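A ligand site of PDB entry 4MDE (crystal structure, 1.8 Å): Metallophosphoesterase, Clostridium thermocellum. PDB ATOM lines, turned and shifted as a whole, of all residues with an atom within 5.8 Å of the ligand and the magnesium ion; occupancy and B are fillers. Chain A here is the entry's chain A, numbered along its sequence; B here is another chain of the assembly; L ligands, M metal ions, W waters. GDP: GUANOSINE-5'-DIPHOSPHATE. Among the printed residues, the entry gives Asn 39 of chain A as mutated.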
ATOM      1  N   GLY A  16       3.878 -17.681   4.128  1.00  0.00           N
ATOM      2  CA  GLY A  16       4.939 -18.598   4.442  1.00  0.00           C
ATOM      3  C   GLY A  16       4.453 -19.950   4.890  1.00  0.00           C
ATOM      4  O   GLY A  16       3.363 -20.083   5.440  1.00  0.00           O
ATOM      5  N   SER A  17       5.294 -20.954   4.665  1.00  0.00           N
ATOM      6  CA  SER A  17       5.022 -22.320   5.071  1.00  0.00           C
ATOM      7  C   SER A  17       4.878 -22.454   6.588  1.00  0.00           C
ATOM      8  O   SER A  17       5.347 -21.597   7.344  1.00  0.00           O
ATOM      9  CB  SER A  17       6.177 -23.209   4.600  1.00  0.00           C
ATOM     10  OG  SER A  17       6.042 -24.525   5.090  1.00  0.00           O
ATOM     11  N   SER A  18       4.236 -23.530   7.027  1.00  0.00           N
ATOM     12  CA  SER A  18       4.357 -23.902   8.413  1.00  0.00           C
ATOM     13  C   SER A  18       5.842 -24.069   8.689  1.00  0.00           C
ATOM     14  O   SER A  18       6.582 -24.583   7.856  1.00  0.00           O
ATOM     15  CB  SER A  18       3.634 -25.221   8.692  1.00  0.00           C
ATOM     16  OG  SER A  18       3.763 -25.537  10.068  1.00  0.00           O
ATOM     17  N   GLY A  19       6.272 -23.594   9.849  1.00  0.00           N
ATOM     18  CA  GLY A  19       7.684 -23.677  10.206  1.00  0.00           C
ATOM     19  C   GLY A  19       8.580 -22.562   9.696  1.00  0.00           C
ATOM     20  O   GLY A  19       9.766 -22.542  10.022  1.00  0.00           O
ATOM     21  N   SER A  20       8.048 -21.623   8.908  1.00  0.00           N
ATOM     22  CA  SER A  20       8.849 -20.501   8.389  1.00  0.00           C
ATOM     23  C   SER A  20       9.090 -19.371   9.412  1.00  0.00           C
ATOM     24  O   SER A  20       9.904 -18.486   9.172  1.00  0.00           O
ATOM     25  CB  SER A  20       8.252 -19.921   7.106  1.00  0.00           C
ATOM     26  OG  SER A  20       6.943 -19.397   7.338  1.00  0.00           O
ATOM     27  N   GLY A  21       8.365 -19.418  10.533  1.00  0.00           N
ATOM     28  CA  GLY A  21       8.567 -18.468  11.612  1.00  0.00           C
ATOM     29  C   GLY A  21       7.618 -17.282  11.629  1.00  0.00           C
ATOM     30  O   GLY A  21       7.918 -16.253  12.240  1.00  0.00           O
ATOM     31  N   LYS A  22       6.454 -17.433  10.993  1.00  0.00           N
ATOM     32  CA  LYS A  22       5.491 -16.343  10.895  1.00  0.00           C
ATOM     33  C   LYS A  22       5.054 -15.798  12.255  1.00  0.00           C
ATOM     34  O   LYS A  22       5.055 -14.585  12.477  1.00  0.00           O
ATOM     35  CB  LYS A  22       4.258 -16.789  10.101  1.00  0.00           C
ATOM     36  CG  LYS A  22       4.578 -17.288   8.692  1.00  0.00           C
ATOM     37  CD  LYS A  22       3.316 -17.674   7.921  1.00  0.00           C
ATOM     38  CE  LYS A  22       2.519 -18.766   8.654  1.00  0.00           C
ATOM     39  NZ  LYS A  22       3.284 -20.040   8.773  1.00  0.00           N
ATOM     40  N   SER A  23       4.649 -16.685  13.155  1.00  0.00           N
ATOM     41  CA  SER A  23       4.110 -16.249  14.432  1.00  0.00           C
ATOM     42  C   SER A  23       5.180 -15.584  15.295  1.00  0.00           C
ATOM     43  O   SER A  23       4.904 -14.592  15.964  1.00  0.00           O
ATOM     44  CB  SER A  23       3.441 -17.414  15.169  1.00  0.00           C
ATOM     45  OG  SER A  23       2.386 -17.906  14.369  1.00  0.00           O
ATOM     46  N   THR A  24       6.386 -16.123  15.263  1.00  0.00           N
ATOM     47  CA  THR A  24       7.507 -15.550  16.017  1.00  0.00           C
ATOM     48  C   THR A  24       7.811 -14.154  15.484  1.00  0.00           C
ATOM     49  O   THR A  24       8.026 -13.208  16.255  1.00  0.00           O
ATOM     50  CB  THR A  24       8.753 -16.445  15.904  1.00  0.00           C
ATOM     51  OG1 THR A  24       8.488 -17.713  16.519  1.00  0.00           O
ATOM     52  CG2 THR A  24       9.949 -15.793  16.585  1.00  0.00           C
ATOM     53  N   PHE A  25       7.801 -14.034  14.165  1.00  0.00           N
ATOM     54  CA  PHE A  25       8.082 -12.760  13.487  1.00  0.00           C
ATOM     55  C   PHE A  25       6.995 -11.756  13.842  1.00  0.00           C
ATOM     56  O   PHE A  25       7.291 -10.600  14.172  1.00  0.00           O
ATOM     57  CB  PHE A  25       8.130 -13.029  11.977  1.00  0.00           C
ATOM     58  CG  PHE A  25       8.290 -11.803  11.116  1.00  0.00           C
ATOM     59  CD1 PHE A  25       7.180 -11.096  10.686  1.00  0.00           C
ATOM     60  CD2 PHE A  25       9.544 -11.416  10.669  1.00  0.00           C
ATOM     61  CE1 PHE A  25       7.315  -9.987   9.864  1.00  0.00           C
ATOM     62  CE2 PHE A  25       9.685 -10.302   9.842  1.00  0.00           C
ATOM     63  CZ  PHE A  25       8.572  -9.588   9.433  1.00  0.00           C
ATOM     64  N   ASN A  39      -4.693 -19.800  13.585  1.00  0.00           N
ATOM     65  CA  ASN A  39      -4.681 -20.824  14.632  1.00  0.00           C
ATOM     66  C   ASN A  39      -5.399 -20.346  15.878  1.00  0.00           C
ATOM     67  O   ASN A  39      -6.152 -21.104  16.475  1.00  0.00           O
ATOM     68  CB  ASN A  39      -3.259 -21.279  14.982  1.00  0.00           C
ATOM     69  CG  ASN A  39      -2.601 -22.070  13.858  1.00  0.00           C
ATOM     70  OD1 ASN A  39      -3.268 -22.761  13.090  1.00  0.00           O
ATOM     71  ND2 ASN A  39      -1.286 -21.992  13.766  1.00  0.00           N
ATOM     72  N   ASP A  79      -1.686 -13.476  10.447  1.00  0.00           N
ATOM     73  CA  ASP A  79      -0.738 -14.540  10.702  1.00  0.00           C
ATOM     74  C   ASP A  79      -1.393 -15.865  10.325  1.00  0.00           C
ATOM     75  O   ASP A  79      -2.058 -16.514  11.142  1.00  0.00           O
ATOM     76  CB  ASP A  79      -0.313 -14.548  12.181  1.00  0.00           C
ATOM     77  CG  ASP A  79       0.632 -15.699  12.511  1.00  0.00           C
ATOM     78  OD1 ASP A  79       1.200 -16.286  11.570  1.00  0.00           O
ATOM     79  OD2 ASP A  79       0.812 -16.001  13.715  1.00  0.00           O
ATOM     80  N   ARG A 117      13.075 -26.613  11.526  1.00  0.00           N
ATOM     81  CA  ARG A 117      12.403 -25.890  12.592  1.00  0.00           C
ATOM     82  C   ARG A 117      11.187 -26.667  13.094  1.00  0.00           C
ATOM     83  O   ARG A 117      10.946 -26.768  14.286  1.00  0.00           O
ATOM     84  CB  ARG A 117      11.993 -24.505  12.115  1.00  0.00           C
ATOM     85  CG  ARG A 117      13.178 -23.598  11.910  1.00  0.00           C
ATOM     86  CD  ARG A 117      12.729 -22.205  11.584  1.00  0.00           C
ATOM     87  NE  ARG A 117      13.852 -21.300  11.330  1.00  0.00           N
ATOM     88  CZ  ARG A 117      13.718 -20.088  10.823  1.00  0.00           C
ATOM     89  NH1 ARG A 117      12.495 -19.651  10.531  1.00  0.00           N
ATOM     90  NH2 ARG A 117      14.776 -19.324  10.599  1.00  0.00           N
ATOM     91  N   ASN A 118      10.439 -27.225  12.153  1.00  0.00           N
ATOM     92  CA  ASN A 118       9.284 -28.048  12.478  1.00  0.00           C
ATOM     93  C   ASN A 118       9.675 -29.257  13.306  1.00  0.00           C
ATOM     94  O   ASN A 118       8.999 -29.614  14.278  1.00  0.00           O
ATOM     95  CB  ASN A 118       8.591 -28.486  11.193  1.00  0.00           C
ATOM     96  CG  ASN A 118       7.376 -29.370  11.453  1.00  0.00           C
ATOM     97  OD1 ASN A 118       6.397 -28.928  12.059  1.00  0.00           O
ATOM     98  ND2 ASN A 118       7.436 -30.601  10.976  1.00  0.00           N
ATOM     99  N   ASN A 120      12.082 -29.440  15.319  1.00  0.00           N
ATOM    100  CA  ASN A 120      12.547 -29.000  16.620  1.00  0.00           C
ATOM    101  C   ASN A 120      11.494 -28.303  17.469  1.00  0.00           C
ATOM    102  O   ASN A 120      11.775 -27.856  18.584  1.00  0.00           O
ATOM    103  CB  ASN A 120      13.771 -28.084  16.465  1.00  0.00           C
ATOM    104  CG  ASN A 120      14.993 -28.825  15.973  1.00  0.00           C
ATOM    105  OD1 ASN A 120      15.327 -29.899  16.471  1.00  0.00           O
ATOM    106  ND2 ASN A 120      15.673 -28.267  14.976  1.00  0.00           N
ATOM    107  N   ARG A 121      10.272 -28.210  16.949  1.00  0.00           N
ATOM    108  CA  ARG A 121       9.172 -27.589  17.701  1.00  0.00           C
ATOM    109  C   ARG A 121       8.824 -28.395  18.947  1.00  0.00           C
ATOM    110  O   ARG A 121       8.815 -29.620  18.924  1.00  0.00           O
ATOM    111  CB  ARG A 121       7.921 -27.455  16.832  1.00  0.00           C
ATOM    112  CG  ARG A 121       8.096 -26.633  15.588  1.00  0.00           C
ATOM    113  CD  ARG A 121       6.765 -26.455  14.875  1.00  0.00           C
ATOM    114  NE  ARG A 121       5.862 -25.628  15.656  1.00  0.00           N
ATOM    115  CZ  ARG A 121       5.141 -24.631  15.160  1.00  0.00           C
ATOM    116  NH1 ARG A 121       5.210 -24.343  13.865  1.00  0.00           N
ATOM    117  NH2 ARG A 121       4.335 -23.934  15.947  1.00  0.00           N
ATOM    118  N   THR A 122       8.539 -27.687  20.034  1.00  0.00           N
ATOM    119  CA  THR A 122       8.095 -28.329  21.271  1.00  0.00           C
ATOM    120  C   THR A 122       6.577 -28.240  21.365  1.00  0.00           C
ATOM    121  O   THR A 122       5.979 -28.679  22.347  1.00  0.00           O
ATOM    122  CB  THR A 122       8.713 -27.656  22.496  1.00  0.00           C
ATOM    123  OG1 THR A 122       8.181 -26.337  22.641  1.00  0.00           O
ATOM    124  CG2 THR A 122      10.235 -27.576  22.350  1.00  0.00           C
ATOM    125  N   ASP A 123       5.987 -27.638  20.344  1.00  0.00           N
ATOM    126  CA  ASP A 123       4.535 -27.534  20.233  1.00  0.00           C
ATOM    127  C   ASP A 123       4.091 -28.387  19.052  1.00  0.00           C
ATOM    128  O   ASP A 123       4.693 -29.424  18.768  1.00  0.00           O
ATOM    129  CB  ASP A 123       4.125 -26.073  20.039  1.00  0.00           C
ATOM    130  CG  ASP A 123       5.028 -25.327  19.066  1.00  0.00           C
ATOM    131  OD1 ASP A 123       5.370 -25.907  18.015  1.00  0.00           O
ATOM    132  OD2 ASP A 123       5.402 -24.177  19.355  1.00  0.00           O
ATOM    133  N   ARG A 124       3.056 -27.932  18.349  1.00  0.00           N
ATOM    134  CA  ARG A 124       2.475 -28.700  17.250  1.00  0.00           C
ATOM    135  C   ARG A 124       3.427 -28.873  16.058  1.00  0.00           C
ATOM    136  O   ARG A 124       3.864 -27.892  15.458  1.00  0.00           O
ATOM    137  CB  ARG A 124       1.166 -28.049  16.784  1.00  0.00           C
ATOM    138  CG  ARG A 124       1.272 -26.547  16.491  1.00  0.00           C
ATOM    139  CD  ARG A 124       1.410 -26.231  15.006  1.00  0.00           C
ATOM    140  NE  ARG A 124       2.043 -24.933  14.783  1.00  0.00           N
ATOM    141  CZ  ARG A 124       1.392 -23.797  14.579  1.00  0.00           C
ATOM    142  NH1 ARG A 124       0.062 -23.781  14.553  1.00  0.00           N
ATOM    143  NH2 ARG A 124       2.050 -22.664  14.408  1.00  0.00           N
ATOM    144  N   PRO A 159      17.194 -16.568   6.480  1.00  0.00           N
ATOM    145  CA  PRO A 159      17.006 -16.223   7.894  1.00  0.00           C
ATOM    146  C   PRO A 159      17.714 -14.924   8.253  1.00  0.00           C
ATOM    147  O   PRO A 159      17.265 -14.184   9.113  1.00  0.00           O
ATOM    148  CB  PRO A 159      17.646 -17.395   8.626  1.00  0.00           C
ATOM    149  CG  PRO A 159      17.491 -18.550   7.671  1.00  0.00           C
ATOM    150  CD  PRO A 159      17.689 -17.935   6.305  1.00  0.00           C
ATOM    151  N   VAL A 162      15.393 -12.125   7.171  1.00  0.00           N
ATOM    152  CA  VAL A 162      14.290 -12.050   8.122  1.00  0.00           C
ATOM    153  C   VAL A 162      14.711 -11.350   9.399  1.00  0.00           C
ATOM    154  O   VAL A 162      13.999 -10.492   9.918  1.00  0.00           O
ATOM    155  CB  VAL A 162      13.739 -13.448   8.478  1.00  0.00           C
ATOM    156  CG1 VAL A 162      12.761 -13.358   9.640  1.00  0.00           C
ATOM    157  CG2 VAL A 162      13.072 -14.079   7.257  1.00  0.00           C
ATOM    158  OP3  DC B   1       1.501 -21.569  12.526  1.00  0.00           O
ATOM    159  P    DC B   1       1.533 -22.376  11.293  1.00  0.00           P
ATOM    160  OP1  DC B   1       2.694 -23.288  11.363  1.00  0.00           O
ATOM    161  OP2  DC B   1       1.384 -21.547  10.086  1.00  0.00           O
ATOM    162  O5'  DC B   1       0.219 -23.297  11.434  1.00  0.00           O
ATOM    163  C5'  DC B   1       0.132 -24.470  10.636  1.00  0.00           C
ATOM    164  C4'  DC B   1      -0.407 -24.185   9.243  1.00  0.00           C
ATOM    165  O4'  DC B   1      -0.357 -25.447   8.528  1.00  0.00           O
ATOM    166  C3'  DC B   1      -1.861 -23.694   9.178  1.00  0.00           C
ATOM    167  O3'  DC B   1      -2.002 -22.822   8.067  1.00  0.00           O
ATOM    168  C2'  DC B   1      -2.603 -25.013   8.966  1.00  0.00           C
ATOM    169  C1'  DC B   1      -1.646 -25.724   8.005  1.00  0.00           C
ATOM    170  N1   DC B   1      -1.853 -27.189   7.957  1.00  0.00           N
ATOM    171  C2   DC B   1      -2.093 -27.797   6.729  1.00  0.00           C
ATOM    172  O2   DC B   1      -2.112 -27.094   5.717  1.00  0.00           O
ATOM    173  N3   DC B   1      -2.315 -29.139   6.686  1.00  0.00           N
ATOM    174  C4   DC B   1      -2.298 -29.849   7.824  1.00  0.00           C
ATOM    175  N4   DC B   1      -2.517 -31.181   7.759  1.00  0.00           N
ATOM    176  C5   DC B   1      -2.057 -29.237   9.090  1.00  0.00           C
ATOM    177  C6   DC B   1      -1.839 -27.908   9.117  1.00  0.00           C
HETATM  178  PB  GDP L   1       5.090 -20.607  12.016  1.00  0.00           P
HETATM  179  O1B GDP L   1       4.014 -19.813  12.707  1.00  0.00           O
HETATM  180  O2B GDP L   1       5.264 -20.152  10.605  1.00  0.00           O
HETATM  181  O3B GDP L   1       4.747 -22.074  12.043  1.00  0.00           O
HETATM  182  O3A GDP L   1       6.509 -20.477  12.765  1.00  0.00           O
HETATM  183  PA  GDP L   1       6.704 -20.239  14.334  1.00  0.00           P
HETATM  184  O1A GDP L   1       5.636 -20.911  15.164  1.00  0.00           O
HETATM  185  O2A GDP L   1       6.876 -18.764  14.624  1.00  0.00           O
HETATM  186  O5' GDP L   1       8.109 -20.987  14.564  1.00  0.00           O
HETATM  187  C5' GDP L   1       8.174 -22.418  14.525  1.00  0.00           C
HETATM  188  C4' GDP L   1       9.475 -22.844  15.176  1.00  0.00           C
HETATM  189  O4' GDP L   1      10.570 -22.174  14.541  1.00  0.00           O
HETATM  190  C3' GDP L   1       9.494 -22.442  16.636  1.00  0.00           C
HETATM  191  O3' GDP L   1      10.133 -23.461  17.399  1.00  0.00           O
HETATM  192  C2' GDP L   1      10.338 -21.188  16.663  1.00  0.00           C
HETATM  193  O2' GDP L   1      10.956 -20.973  17.945  1.00  0.00           O
HETATM  194  C1' GDP L   1      11.304 -21.427  15.512  1.00  0.00           C
HETATM  195  N9  GDP L   1      11.697 -20.124  14.942  1.00  0.00           N
HETATM  196  C8  GDP L   1      10.844 -19.133  14.605  1.00  0.00           C
HETATM  197  N7  GDP L   1      11.523 -18.058  14.104  1.00  0.00           N
HETATM  198  C5  GDP L   1      12.826 -18.382  14.105  1.00  0.00           C
HETATM  199  C6  GDP L   1      14.083 -17.701  13.714  1.00  0.00           C
HETATM  200  O6  GDP L   1      14.035 -16.546  13.248  1.00  0.00           O
HETATM  201  N1  GDP L   1      15.238 -18.351  13.870  1.00  0.00           N
HETATM  202  C2  GDP L   1      15.277 -19.601  14.380  1.00  0.00           C
HETATM  203  N2  GDP L   1      16.466 -20.230  14.523  1.00  0.00           N
HETATM  204  N3  GDP L   1      14.163 -20.286  14.765  1.00  0.00           N
HETATM  205  C4  GDP L   1      12.941 -19.735  14.657  1.00  0.00           C
HETATM  206 MG    MG M   1       2.158 -19.826  13.469  1.00  0.00          MG
HETATM  207  O   HOH W   1      10.701 -15.571  12.347  1.00  0.00           O
HETATM  208  O   HOH W   2      12.054 -25.024  16.187  1.00  0.00           O
HETATM  209  O   HOH W   3      15.922 -15.385  11.135  1.00  0.00           O
HETATM  210  O   HOH W   4       0.204 -19.647  14.480  1.00  0.00           O
HETATM  211  O   HOH W   5       1.352 -18.773  11.822  1.00  0.00           O
HETATM  212  O   HOH W   6      12.833 -22.438  19.177  1.00  0.00           O
HETATM  213  O   HOH W   7       2.942 -20.761  15.262  1.00  0.00           O
HETATM  214  O   HOH W   8       5.923 -21.064  17.888  1.00  0.00           O
HETATM  215  O   HOH W   9       8.645 -24.254  19.605  1.00  0.00           O
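The guanidinium group (NH2) of Arg 117 sits close to a nitrogen (N1) of the ligand (3.4 Å).
Residues that only touch the ligand: Ser 17 and Ser 20.
11 residues have an atom within 4 Å of the ligand: Ser 17, Gly 19, Ser 20, Gly 21, Lys 22, Ser 23, Thr 24, Arg 117, Arg 121, Arg 124 and DC 1 of chain B.
Water W5 bridges the side-chain carboxylate (OD1) of Asp 79 (2.5 Å) and OP2 of DC 1 of chain B (3.3 Å).
Water W8 lies within hydrogen-bond range of an oxygen (O1A) of the ligand and the side-chain carboxylate of Asp 123.
Water W2 lies within hydrogen-bond range of an oxygen (O3') of the ligand (2.8 Å) and the backbone carbonyl oxygen (O) of Arg 117 (2.8 Å).
Water W9 lies within hydrogen-bond range of an oxygen (O3') of the ligand (2.8 Å), the side-chain carboxylate (OD2) of Asp 123 (3.3 Å) and the backbone NH (N) of Thr 122 (3.5 Å).
Water W3 bridges the backbone carbonyl oxygen of Pro 159 and an oxygen (O6) of the ligand.
Water W1 bridges the backbone carbonyl oxygen (O) of Gly 21 (2.9 Å) and a nitrogen (N7) of the ligand (3.2 Å).
The magnesium ion is bound by an oxygen (O1B) of the ligand (2.0 Å), OP3 of DC 1 of chain B (2.1 Å), water W5 (2.1 Å), the side-chain hydroxyl (OG) of Ser 23 (2.1 Å), water W7 (2.2 Å) and water W4 (2.2 Å).
The magnesium ion has six donor atoms within binding distance.
An oxygen (O2A) of the ligand is in hydrogen-bond range of the backbone NH (N) of Ser 23 (3.4 Å).
The backbone NH (N) of Lys 22 lies within hydrogen-bond range of an oxygen (O2B) of the ligand (3.0 Å).
The side-chain amino group (NZ) of Lys 22 is in salt-bridge range of an oxygen (O2B) of the ligand, 2.7 Å away.
O2A of the ligand sits at hydrogen-bond distance from N of Thr 24 (2.8 Å).
An oxygen (O2A) of the ligand is in hydrogen-bond range of the side-chain hydroxyl (OG1) of Thr 24 (2.7 Å).
NH1 of Arg 121 is in salt-bridge range of O3B of the ligand (2.9 Å).
NH2 of Arg 124 is in salt-bridge range of O3B of the ligand (3.6 Å).
N of Gly 19 is in hydrogen-bond range of O3B of the ligand (3.1 Å).
The backbone NH (N) of Gly 21 sits at hydrogen-bond distance from an oxygen (O3A) of the ligand.
Merely in contact with the magnesium ion: Arg 124.
The nearest printed residue that does not touch the magnesium ion is Asp 79 (4.1 Å).
OP2 of DC 1 of chain B is in salt-bridge range of the side-chain amino group (NZ) of Lys 22 (2.8 Å).
OP1 of DC 1 of chain B is in salt-bridge range of the guanidinium group of Arg 121, at 3.7 Å.
NZ of Lys 22 sits at hydrogen-bond distance from O of Ser 17, 3.0 Å away.
The side-chain amino group (NZ) of Lys 22 lies within hydrogen-bond range of the backbone carbonyl oxygen (O) of Gly 16 (3.3 Å).
The guanidinium group (NE) of Arg 121 is in hydrogen-bond range of the backbone carbonyl oxygen (O) of Arg 124 (3.0 Å).
The side-chain carboxylate (OD1) of Asp 123 lies within salt-bridge range of the guanidinium group (NE) of Arg 121, 2.4 Å away.
The guanidinium group (NH1) of Arg 117 sits at hydrogen-bond distance from the backbone carbonyl oxygen (O) of Ser 20 (3.1 Å).
The backbone carbonyl oxygen (O) of Ser 17 lies within hydrogen-bond range of the side-chain hydroxyl (OG) of Ser 20, at 2.7 Å.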
